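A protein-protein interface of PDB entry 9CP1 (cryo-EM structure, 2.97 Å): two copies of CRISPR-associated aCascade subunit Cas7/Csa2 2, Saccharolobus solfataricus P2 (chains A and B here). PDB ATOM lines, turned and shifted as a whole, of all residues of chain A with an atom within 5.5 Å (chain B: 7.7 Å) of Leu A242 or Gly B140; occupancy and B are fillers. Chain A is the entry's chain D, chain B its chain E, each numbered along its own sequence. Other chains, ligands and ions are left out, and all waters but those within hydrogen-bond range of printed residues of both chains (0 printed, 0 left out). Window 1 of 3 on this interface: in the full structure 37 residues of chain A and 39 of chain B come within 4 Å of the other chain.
Printed residues of chain B that touch a printed residue of chain A: Ala B54, Lys B138, Leu B139, Gly B140, Tyr B141, Ile B143, Ser B187 and Met B260. Hydrophobic or aromatic side chains of chain B within 4 Å of the printed part of chain A: Ala B54, Tyr B141, Ile B143 and Met B260. Of the 9 printed residues of chain A, 6 touch a printed residue of chain B. Printed residues of chain A that touch a printed residue of chain B: Leu A12, Arg A238, Ser A239, Arg A240, Phe A241 and Leu A242. Among the printed residues, no Asp or Glu carboxylate lies within 4 Å of a Lys or Arg side-chain nitrogen of the other chain.
Of chain B, only Leu B139 (3.1 Å), Gly B140 (3.8 Å) and Ser B187 (3.8 Å) come within 4 Å of Leu A242. No residue of chain B comes within 4 Å of Pro A243. Printed residues of chain B within 4 Å of Ser A239: Lys B138 and Leu B139. Of the printed residues of chain A, Lys B138 touches Arg A238 and Ser A239. Of the printed residues of chain B, Phe A241 touches Leu B139 and Tyr B141. The nearest residue of chain B that does not touch Leu A242 is Lys B138 (4.5 Å). The nearest residue of chain A that does not touch Gly B140 is Phe A241 (4.6 Å).
No position is printed for both chains. Of the 14 pairs that touch across the chains among the printed residues, none has its exchanged pair printed and touching as well.
Among the printed residues, pairs that only touch across the chains: Ser A239 with Lys B138 (3.2 Å), Arg A238 with Lys B138 (3.4 Å), Arg A240 with Ala B54 (3.4 Å), Phe A241 with Tyr B141 (3.5 Å), Leu A12 with Tyr B141 (3.5 Å), Leu A12 with Ile B143 (3.5 Å), Leu A242 with Gly B140 (3.8 Å), Leu A242 with Ser B187 (3.8 Å) and Arg A240 with Gly B140 (3.9 Å).
The backbone carbonyl oxygen (O) of Glu B189 lies within hydrogen-bond range of the backbone NH (N) of Lys B138 (3.0 Å). O of Ile B143 lies within hydrogen-bond range of N of Thr B185 (2.9 Å).
The backbone carbonyl oxygen (O) of Arg A240 sits close to the backbone carbonyl oxygen (O) of Leu B139, 3.4 Å away. N of Leu A242 is in hydrogen-bond range of O of Leu B139, at 3.1 Å. The backbone NH of Leu B139 sits at hydrogen-bond distance from the backbone carbonyl oxygen of Ser A239 (2.8 Å). O of Leu B139 is in hydrogen-bond range of N of Phe A241, 3.5 Å away. SD of Met B260 sits at hydrogen-bond distance from NH2 of Arg A238 (3.5 Å).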
ATOM      1  N   LEU A  12       8.662 -34.010  -4.703  1.00  0.00           N
ATOM      2  CA  LEU A  12       7.426 -33.270  -4.443  1.00  0.00           C
ATOM      3  C   LEU A  12       7.561 -31.812  -4.893  1.00  0.00           C
ATOM      4  O   LEU A  12       7.568 -30.870  -4.103  1.00  0.00           O
ATOM      5  CB  LEU A  12       7.024 -33.372  -2.968  1.00  0.00           C
ATOM      6  CG  LEU A  12       6.036 -34.504  -2.678  1.00  0.00           C
ATOM      7  CD1 LEU A  12       6.618 -35.848  -3.067  1.00  0.00           C
ATOM      8  CD2 LEU A  12       5.627 -34.508  -1.228  1.00  0.00           C
ATOM      9  N   LYS A 237       6.241 -21.044  -7.699  1.00  0.00           N
ATOM     10  CA  LYS A 237       5.380 -21.692  -6.712  1.00  0.00           C
ATOM     11  C   LYS A 237       6.181 -22.149  -5.496  1.00  0.00           C
ATOM     12  O   LYS A 237       5.976 -23.243  -4.969  1.00  0.00           O
ATOM     13  CB  LYS A 237       4.612 -22.860  -7.331  1.00  0.00           C
ATOM     14  CG  LYS A 237       3.317 -22.446  -8.001  1.00  0.00           C
ATOM     15  CD  LYS A 237       2.594 -23.632  -8.605  1.00  0.00           C
ATOM     16  CE  LYS A 237       1.479 -23.174  -9.524  1.00  0.00           C
ATOM     17  NZ  LYS A 237       0.439 -24.222  -9.686  1.00  0.00           N
ATOM     18  N   ARG A 238       7.108 -21.304  -5.055  1.00  0.00           N
ATOM     19  CA  ARG A 238       7.940 -21.599  -3.899  1.00  0.00           C
ATOM     20  C   ARG A 238       7.290 -21.207  -2.583  1.00  0.00           C
ATOM     21  O   ARG A 238       7.861 -21.481  -1.523  1.00  0.00           O
ATOM     22  CB  ARG A 238       9.288 -20.885  -4.024  1.00  0.00           C
ATOM     23  CG  ARG A 238      10.161 -21.392  -5.154  1.00  0.00           C
ATOM     24  CD  ARG A 238      11.409 -20.541  -5.304  1.00  0.00           C
ATOM     25  NE  ARG A 238      12.356 -20.769  -4.221  1.00  0.00           N
ATOM     26  CZ  ARG A 238      13.254 -21.745  -4.204  1.00  0.00           C
ATOM     27  NH1 ARG A 238      13.364 -22.599  -5.207  1.00  0.00           N
ATOM     28  NH2 ARG A 238      14.062 -21.864  -3.155  1.00  0.00           N
ATOM     29  N   SER A 239       6.121 -20.566  -2.617  1.00  0.00           N
ATOM     30  CA  SER A 239       5.495 -20.117  -1.379  1.00  0.00           C
ATOM     31  C   SER A 239       4.869 -21.276  -0.613  1.00  0.00           C
ATOM     32  O   SER A 239       4.973 -21.340   0.616  1.00  0.00           O
ATOM     33  CB  SER A 239       4.451 -19.046  -1.683  1.00  0.00           C
ATOM     34  OG  SER A 239       3.389 -19.580  -2.447  1.00  0.00           O
ATOM     35  N   ARG A 240       4.213 -22.200  -1.311  1.00  0.00           N
ATOM     36  CA  ARG A 240       3.554 -23.319  -0.660  1.00  0.00           C
ATOM     37  C   ARG A 240       4.041 -24.681  -1.129  1.00  0.00           C
ATOM     38  O   ARG A 240       3.608 -25.695  -0.571  1.00  0.00           O
ATOM     39  CB  ARG A 240       2.035 -23.236  -0.865  1.00  0.00           C
ATOM     40  CG  ARG A 240       1.426 -21.920  -0.418  1.00  0.00           C
ATOM     41  CD  ARG A 240       1.220 -21.880   1.083  1.00  0.00           C
ATOM     42  NE  ARG A 240       0.822 -20.553   1.534  1.00  0.00           N
ATOM     43  CZ  ARG A 240       1.657 -19.646   2.015  1.00  0.00           C
ATOM     44  NH1 ARG A 240       2.952 -19.891   2.126  1.00  0.00           N
ATOM     45  NH2 ARG A 240       1.185 -18.462   2.391  1.00  0.00           N
ATOM     46  N   PHE A 241       4.911 -24.738  -2.131  1.00  0.00           N
ATOM     47  CA  PHE A 241       5.455 -25.980  -2.670  1.00  0.00           C
ATOM     48  C   PHE A 241       6.975 -25.929  -2.679  1.00  0.00           C
ATOM     49  O   PHE A 241       7.624 -26.198  -3.690  1.00  0.00           O
ATOM     50  CB  PHE A 241       4.931 -26.269  -4.072  1.00  0.00           C
ATOM     51  CG  PHE A 241       3.444 -26.461  -4.139  1.00  0.00           C
ATOM     52  CD1 PHE A 241       2.882 -27.695  -3.867  1.00  0.00           C
ATOM     53  CD2 PHE A 241       2.610 -25.409  -4.468  1.00  0.00           C
ATOM     54  CE1 PHE A 241       1.517 -27.876  -3.924  1.00  0.00           C
ATOM     55  CE2 PHE A 241       1.242 -25.588  -4.529  1.00  0.00           C
ATOM     56  CZ  PHE A 241       0.697 -26.820  -4.255  1.00  0.00           C
ATOM     57  N   LEU A 242       7.560 -25.553  -1.551  1.00  0.00           N
ATOM     58  CA  LEU A 242       9.009 -25.484  -1.441  1.00  0.00           C
ATOM     59  C   LEU A 242       9.609 -26.872  -1.640  1.00  0.00           C
ATOM     60  O   LEU A 242       9.256 -27.803  -0.900  1.00  0.00           O
ATOM     61  CB  LEU A 242       9.403 -24.923  -0.080  1.00  0.00           C
ATOM     62  CG  LEU A 242      10.843 -24.449   0.094  1.00  0.00           C
ATOM     63  CD1 LEU A 242      11.010 -23.060  -0.473  1.00  0.00           C
ATOM     64  CD2 LEU A 242      11.221 -24.470   1.558  1.00  0.00           C
ATOM     65  N   PRO A 243      10.503 -27.058  -2.606  1.00  0.00           N
ATOM     66  CA  PRO A 243      11.006 -28.398  -2.905  1.00  0.00           C
ATOM     67  C   PRO A 243      12.123 -28.819  -1.964  1.00  0.00           C
ATOM     68  O   PRO A 243      12.684 -28.024  -1.210  1.00  0.00           O
ATOM     69  CB  PRO A 243      11.522 -28.262  -4.338  1.00  0.00           C
ATOM     70  CG  PRO A 243      11.960 -26.849  -4.424  1.00  0.00           C
ATOM     71  CD  PRO A 243      11.063 -26.044  -3.515  1.00  0.00           C
ATOM     72  N   SER A 244      12.438 -30.110  -2.031  1.00  0.00           N
ATOM     73  CA  SER A 244      13.506 -30.721  -1.247  1.00  0.00           C
ATOM     74  C   SER A 244      14.635 -31.104  -2.194  1.00  0.00           C
ATOM     75  O   SER A 244      14.579 -32.156  -2.838  1.00  0.00           O
ATOM     76  CB  SER A 244      12.983 -31.939  -0.491  1.00  0.00           C
ATOM     77  OG  SER A 244      14.030 -32.602   0.186  1.00  0.00           O
ATOM     78  N   GLY B   4      14.835 -22.429   8.410  1.00  0.00           N
ATOM     79  CA  GLY B   4      14.864 -23.497   9.389  1.00  0.00           C
ATOM     80  C   GLY B   4      14.585 -24.852   8.782  1.00  0.00           C
ATOM     81  O   GLY B   4      13.856 -24.981   7.796  1.00  0.00           O
ATOM     82  N   ILE B  48       1.760 -34.817   3.905  1.00  0.00           N
ATOM     83  CA  ILE B  48       0.851 -33.772   4.363  1.00  0.00           C
ATOM     84  C   ILE B  48       1.210 -32.483   3.641  1.00  0.00           C
ATOM     85  O   ILE B  48       2.368 -32.054   3.673  1.00  0.00           O
ATOM     86  CB  ILE B  48       0.926 -33.571   5.887  1.00  0.00           C
ATOM     87  CG1 ILE B  48       0.330 -34.774   6.613  1.00  0.00           C
ATOM     88  CG2 ILE B  48       0.199 -32.304   6.288  1.00  0.00           C
ATOM     89  CD1 ILE B  48       0.818 -34.921   8.029  1.00  0.00           C
ATOM     90  N   SER B  49       0.222 -31.860   3.009  1.00  0.00           N
ATOM     91  CA  SER B  49       0.491 -30.690   2.189  1.00  0.00           C
ATOM     92  C   SER B  49       0.850 -29.487   3.053  1.00  0.00           C
ATOM     93  O   SER B  49       0.617 -29.462   4.264  1.00  0.00           O
ATOM     94  CB  SER B  49      -0.715 -30.351   1.319  1.00  0.00           C
ATOM     95  OG  SER B  49      -1.670 -29.614   2.059  1.00  0.00           O
ATOM     96  N   GLY B  50       1.430 -28.475   2.407  1.00  0.00           N
ATOM     97  CA  GLY B  50       1.836 -27.265   3.096  1.00  0.00           C
ATOM     98  C   GLY B  50       0.747 -26.236   3.298  1.00  0.00           C
ATOM     99  O   GLY B  50       0.925 -25.314   4.100  1.00  0.00           O
ATOM    100  N   GLU B  51      -0.379 -26.369   2.597  1.00  0.00           N
ATOM    101  CA  GLU B  51      -1.441 -25.380   2.735  1.00  0.00           C
ATOM    102  C   GLU B  51      -2.143 -25.490   4.082  1.00  0.00           C
ATOM    103  O   GLU B  51      -2.596 -24.476   4.626  1.00  0.00           O
ATOM    104  CB  GLU B  51      -2.434 -25.513   1.586  1.00  0.00           C
ATOM    105  CG  GLU B  51      -1.913 -24.922   0.286  1.00  0.00           C
ATOM    106  CD  GLU B  51      -2.925 -24.981  -0.835  1.00  0.00           C
ATOM    107  OE1 GLU B  51      -3.934 -25.699  -0.686  1.00  0.00           O
ATOM    108  OE2 GLU B  51      -2.714 -24.310  -1.867  1.00  0.00           O
ATOM    109  N   LEU B  53      -0.516 -26.220   6.818  1.00  0.00           N
ATOM    110  CA  LEU B  53       0.421 -25.484   7.658  1.00  0.00           C
ATOM    111  C   LEU B  53       0.252 -23.982   7.481  1.00  0.00           C
ATOM    112  O   LEU B  53       0.316 -23.223   8.456  1.00  0.00           O
ATOM    113  CB  LEU B  53       1.852 -25.898   7.326  1.00  0.00           C
ATOM    114  CG  LEU B  53       2.116 -27.397   7.188  1.00  0.00           C
ATOM    115  CD1 LEU B  53       3.542 -27.630   6.736  1.00  0.00           C
ATOM    116  CD2 LEU B  53       1.843 -28.112   8.496  1.00  0.00           C
ATOM    117  N   ALA B  54       0.046 -23.534   6.240  1.00  0.00           N
ATOM    118  CA  ALA B  54      -0.183 -22.113   6.002  1.00  0.00           C
ATOM    119  C   ALA B  54      -1.434 -21.631   6.723  1.00  0.00           C
ATOM    120  O   ALA B  54      -1.435 -20.549   7.325  1.00  0.00           O
ATOM    121  CB  ALA B  54      -0.289 -21.841   4.503  1.00  0.00           C
ATOM    122  N   LYS B 138       7.305 -19.024   3.390  1.00  0.00           N
ATOM    123  CA  LYS B 138       7.332 -20.090   2.398  1.00  0.00           C
ATOM    124  C   LYS B 138       7.442 -21.443   3.086  1.00  0.00           C
ATOM    125  O   LYS B 138       8.320 -21.648   3.929  1.00  0.00           O
ATOM    126  CB  LYS B 138       8.484 -19.881   1.416  1.00  0.00           C
ATOM    127  CG  LYS B 138       8.362 -18.577   0.655  1.00  0.00           C
ATOM    128  CD  LYS B 138       9.410 -18.429  -0.424  1.00  0.00           C
ATOM    129  CE  LYS B 138       9.248 -17.098  -1.139  1.00  0.00           C
ATOM    130  NZ  LYS B 138      10.198 -16.944  -2.273  1.00  0.00           N
ATOM    131  N   LEU B 139       6.555 -22.361   2.715  1.00  0.00           N
ATOM    132  CA  LEU B 139       6.457 -23.676   3.326  1.00  0.00           C
ATOM    133  C   LEU B 139       6.440 -24.733   2.229  1.00  0.00           C
ATOM    134  O   LEU B 139       6.353 -24.420   1.039  1.00  0.00           O
ATOM    135  CB  LEU B 139       5.201 -23.779   4.198  1.00  0.00           C
ATOM    136  CG  LEU B 139       5.157 -22.882   5.433  1.00  0.00           C
ATOM    137  CD1 LEU B 139       3.808 -22.990   6.114  1.00  0.00           C
ATOM    138  CD2 LEU B 139       6.266 -23.224   6.394  1.00  0.00           C
ATOM    139  N   GLY B 140       6.514 -25.999   2.637  1.00  0.00           N
ATOM    140  CA  GLY B 140       6.492 -27.102   1.700  1.00  0.00           C
ATOM    141  C   GLY B 140       5.769 -28.296   2.284  1.00  0.00           C
ATOM    142  O   GLY B 140       5.291 -28.265   3.418  1.00  0.00           O
ATOM    143  N   TYR B 141       5.691 -29.359   1.487  1.00  0.00           N
ATOM    144  CA  TYR B 141       5.069 -30.593   1.943  1.00  0.00           C
ATOM    145  C   TYR B 141       5.861 -31.197   3.094  1.00  0.00           C
ATOM    146  O   TYR B 141       7.049 -30.918   3.274  1.00  0.00           O
ATOM    147  CB  TYR B 141       4.980 -31.604   0.803  1.00  0.00           C
ATOM    148  CG  TYR B 141       3.735 -31.504  -0.044  1.00  0.00           C
ATOM    149  CD1 TYR B 141       3.432 -30.346  -0.734  1.00  0.00           C
ATOM    150  CD2 TYR B 141       2.868 -32.579  -0.161  1.00  0.00           C
ATOM    151  CE1 TYR B 141       2.297 -30.257  -1.512  1.00  0.00           C
ATOM    152  CE2 TYR B 141       1.733 -32.500  -0.934  1.00  0.00           C
ATOM    153  CZ  TYR B 141       1.453 -31.337  -1.608  1.00  0.00           C
ATOM    154  OH  TYR B 141       0.321 -31.253  -2.381  1.00  0.00           O
ATOM    155  N   MET B 142       5.192 -32.031   3.882  1.00  0.00           N
ATOM    156  CA  MET B 142       5.809 -32.704   5.018  1.00  0.00           C
ATOM    157  C   MET B 142       6.060 -34.162   4.645  1.00  0.00           C
ATOM    158  O   MET B 142       5.139 -34.983   4.664  1.00  0.00           O
ATOM    159  CB  MET B 142       4.928 -32.587   6.260  1.00  0.00           C
ATOM    160  CG  MET B 142       5.642 -32.943   7.548  1.00  0.00           C
ATOM    161  SD  MET B 142       4.640 -32.703   9.023  1.00  0.00           S
ATOM    162  CE  MET B 142       4.889 -30.955   9.309  1.00  0.00           C
ATOM    163  N   ILE B 143       7.310 -34.478   4.318  1.00  0.00           N
ATOM    164  CA  ILE B 143       7.701 -35.803   3.844  1.00  0.00           C
ATOM    165  C   ILE B 143       8.494 -36.509   4.937  1.00  0.00           C
ATOM    166  O   ILE B 143       9.233 -35.848   5.681  1.00  0.00           O
ATOM    167  CB  ILE B 143       8.531 -35.699   2.555  1.00  0.00           C
ATOM    168  CG1 ILE B 143       7.826 -34.814   1.536  1.00  0.00           C
ATOM    169  CG2 ILE B 143       8.802 -37.065   1.956  1.00  0.00           C
ATOM    170  CD1 ILE B 143       8.778 -34.062   0.641  1.00  0.00           C
ATOM    171  N   THR B 185       9.852 -34.628   8.222  1.00  0.00           N
ATOM    172  CA  THR B 185      10.818 -33.540   8.180  1.00  0.00           C
ATOM    173  C   THR B 185      10.287 -32.444   7.274  1.00  0.00           C
ATOM    174  O   THR B 185       9.632 -32.724   6.267  1.00  0.00           O
ATOM    175  CB  THR B 185      12.189 -33.991   7.657  1.00  0.00           C
ATOM    176  OG1 THR B 185      12.061 -34.428   6.300  1.00  0.00           O
ATOM    177  CG2 THR B 185      12.760 -35.118   8.502  1.00  0.00           C
ATOM    178  N   PHE B 186      10.577 -31.194   7.627  1.00  0.00           N
ATOM    179  CA  PHE B 186      10.203 -30.101   6.738  1.00  0.00           C
ATOM    180  C   PHE B 186      11.031 -28.865   7.049  1.00  0.00           C
ATOM    181  O   PHE B 186      11.602 -28.729   8.133  1.00  0.00           O
ATOM    182  CB  PHE B 186       8.704 -29.783   6.824  1.00  0.00           C
ATOM    183  CG  PHE B 186       8.337 -28.861   7.947  1.00  0.00           C
ATOM    184  CD1 PHE B 186       8.186 -29.342   9.234  1.00  0.00           C
ATOM    185  CD2 PHE B 186       8.127 -27.514   7.712  1.00  0.00           C
ATOM    186  CE1 PHE B 186       7.844 -28.496  10.265  1.00  0.00           C
ATOM    187  CE2 PHE B 186       7.787 -26.663   8.739  1.00  0.00           C
ATOM    188  CZ  PHE B 186       7.644 -27.155  10.016  1.00  0.00           C
ATOM    189  N   SER B 187      11.065 -27.952   6.083  1.00  0.00           N
ATOM    190  CA  SER B 187      11.850 -26.733   6.176  1.00  0.00           C
ATOM    191  C   SER B 187      10.968 -25.529   5.876  1.00  0.00           C
ATOM    192  O   SER B 187       9.937 -25.639   5.210  1.00  0.00           O
ATOM    193  CB  SER B 187      13.047 -26.768   5.219  1.00  0.00           C
ATOM    194  OG  SER B 187      12.631 -27.072   3.899  1.00  0.00           O
ATOM    195  N   PHE B 188      11.391 -24.371   6.376  1.00  0.00           N
ATOM    196  CA  PHE B 188      10.618 -23.145   6.243  1.00  0.00           C
ATOM    197  C   PHE B 188      11.550 -21.957   6.061  1.00  0.00           C
ATOM    198  O   PHE B 188      12.733 -22.009   6.408  1.00  0.00           O
ATOM    199  CB  PHE B 188       9.712 -22.916   7.456  1.00  0.00           C
ATOM    200  CG  PHE B 188      10.446 -22.480   8.687  1.00  0.00           C
ATOM    201  CD1 PHE B 188      10.989 -23.414   9.549  1.00  0.00           C
ATOM    202  CD2 PHE B 188      10.587 -21.137   8.987  1.00  0.00           C
ATOM    203  CE1 PHE B 188      11.660 -23.019  10.682  1.00  0.00           C
ATOM    204  CE2 PHE B 188      11.262 -20.736  10.117  1.00  0.00           C
ATOM    205  CZ  PHE B 188      11.799 -21.678  10.966  1.00  0.00           C
ATOM    206  N   GLU B 189      10.986 -20.870   5.536  1.00  0.00           N
ATOM    207  CA  GLU B 189      11.725 -19.647   5.256  1.00  0.00           C
ATOM    208  C   GLU B 189      10.833 -18.442   5.523  1.00  0.00           C
ATOM    209  O   GLU B 189       9.633 -18.478   5.243  1.00  0.00           O
ATOM    210  CB  GLU B 189      12.224 -19.632   3.805  1.00  0.00           C
ATOM    211  CG  GLU B 189      12.712 -18.285   3.311  1.00  0.00           C
ATOM    212  CD  GLU B 189      13.375 -18.373   1.953  1.00  0.00           C
ATOM    213  OE1 GLU B 189      14.113 -19.351   1.714  1.00  0.00           O
ATOM    214  OE2 GLU B 189      13.160 -17.464   1.123  1.00  0.00           O
ATOM    215  N   MET B 260      19.936 -21.435   2.265  1.00  0.00           N
ATOM    216  CA  MET B 260      19.000 -22.542   2.409  1.00  0.00           C
ATOM    217  C   MET B 260      19.668 -23.701   3.136  1.00  0.00           C
ATOM    218  O   MET B 260      20.595 -24.320   2.601  1.00  0.00           O
ATOM    219  CB  MET B 260      18.490 -22.995   1.042  1.00  0.00           C
ATOM    220  CG  MET B 260      17.460 -22.063   0.430  1.00  0.00           C
ATOM    221  SD  MET B 260      16.675 -22.760  -1.034  1.00  0.00           S
ATOM    222  CE  MET B 260      18.107 -23.067  -2.062  1.00  0.00           C
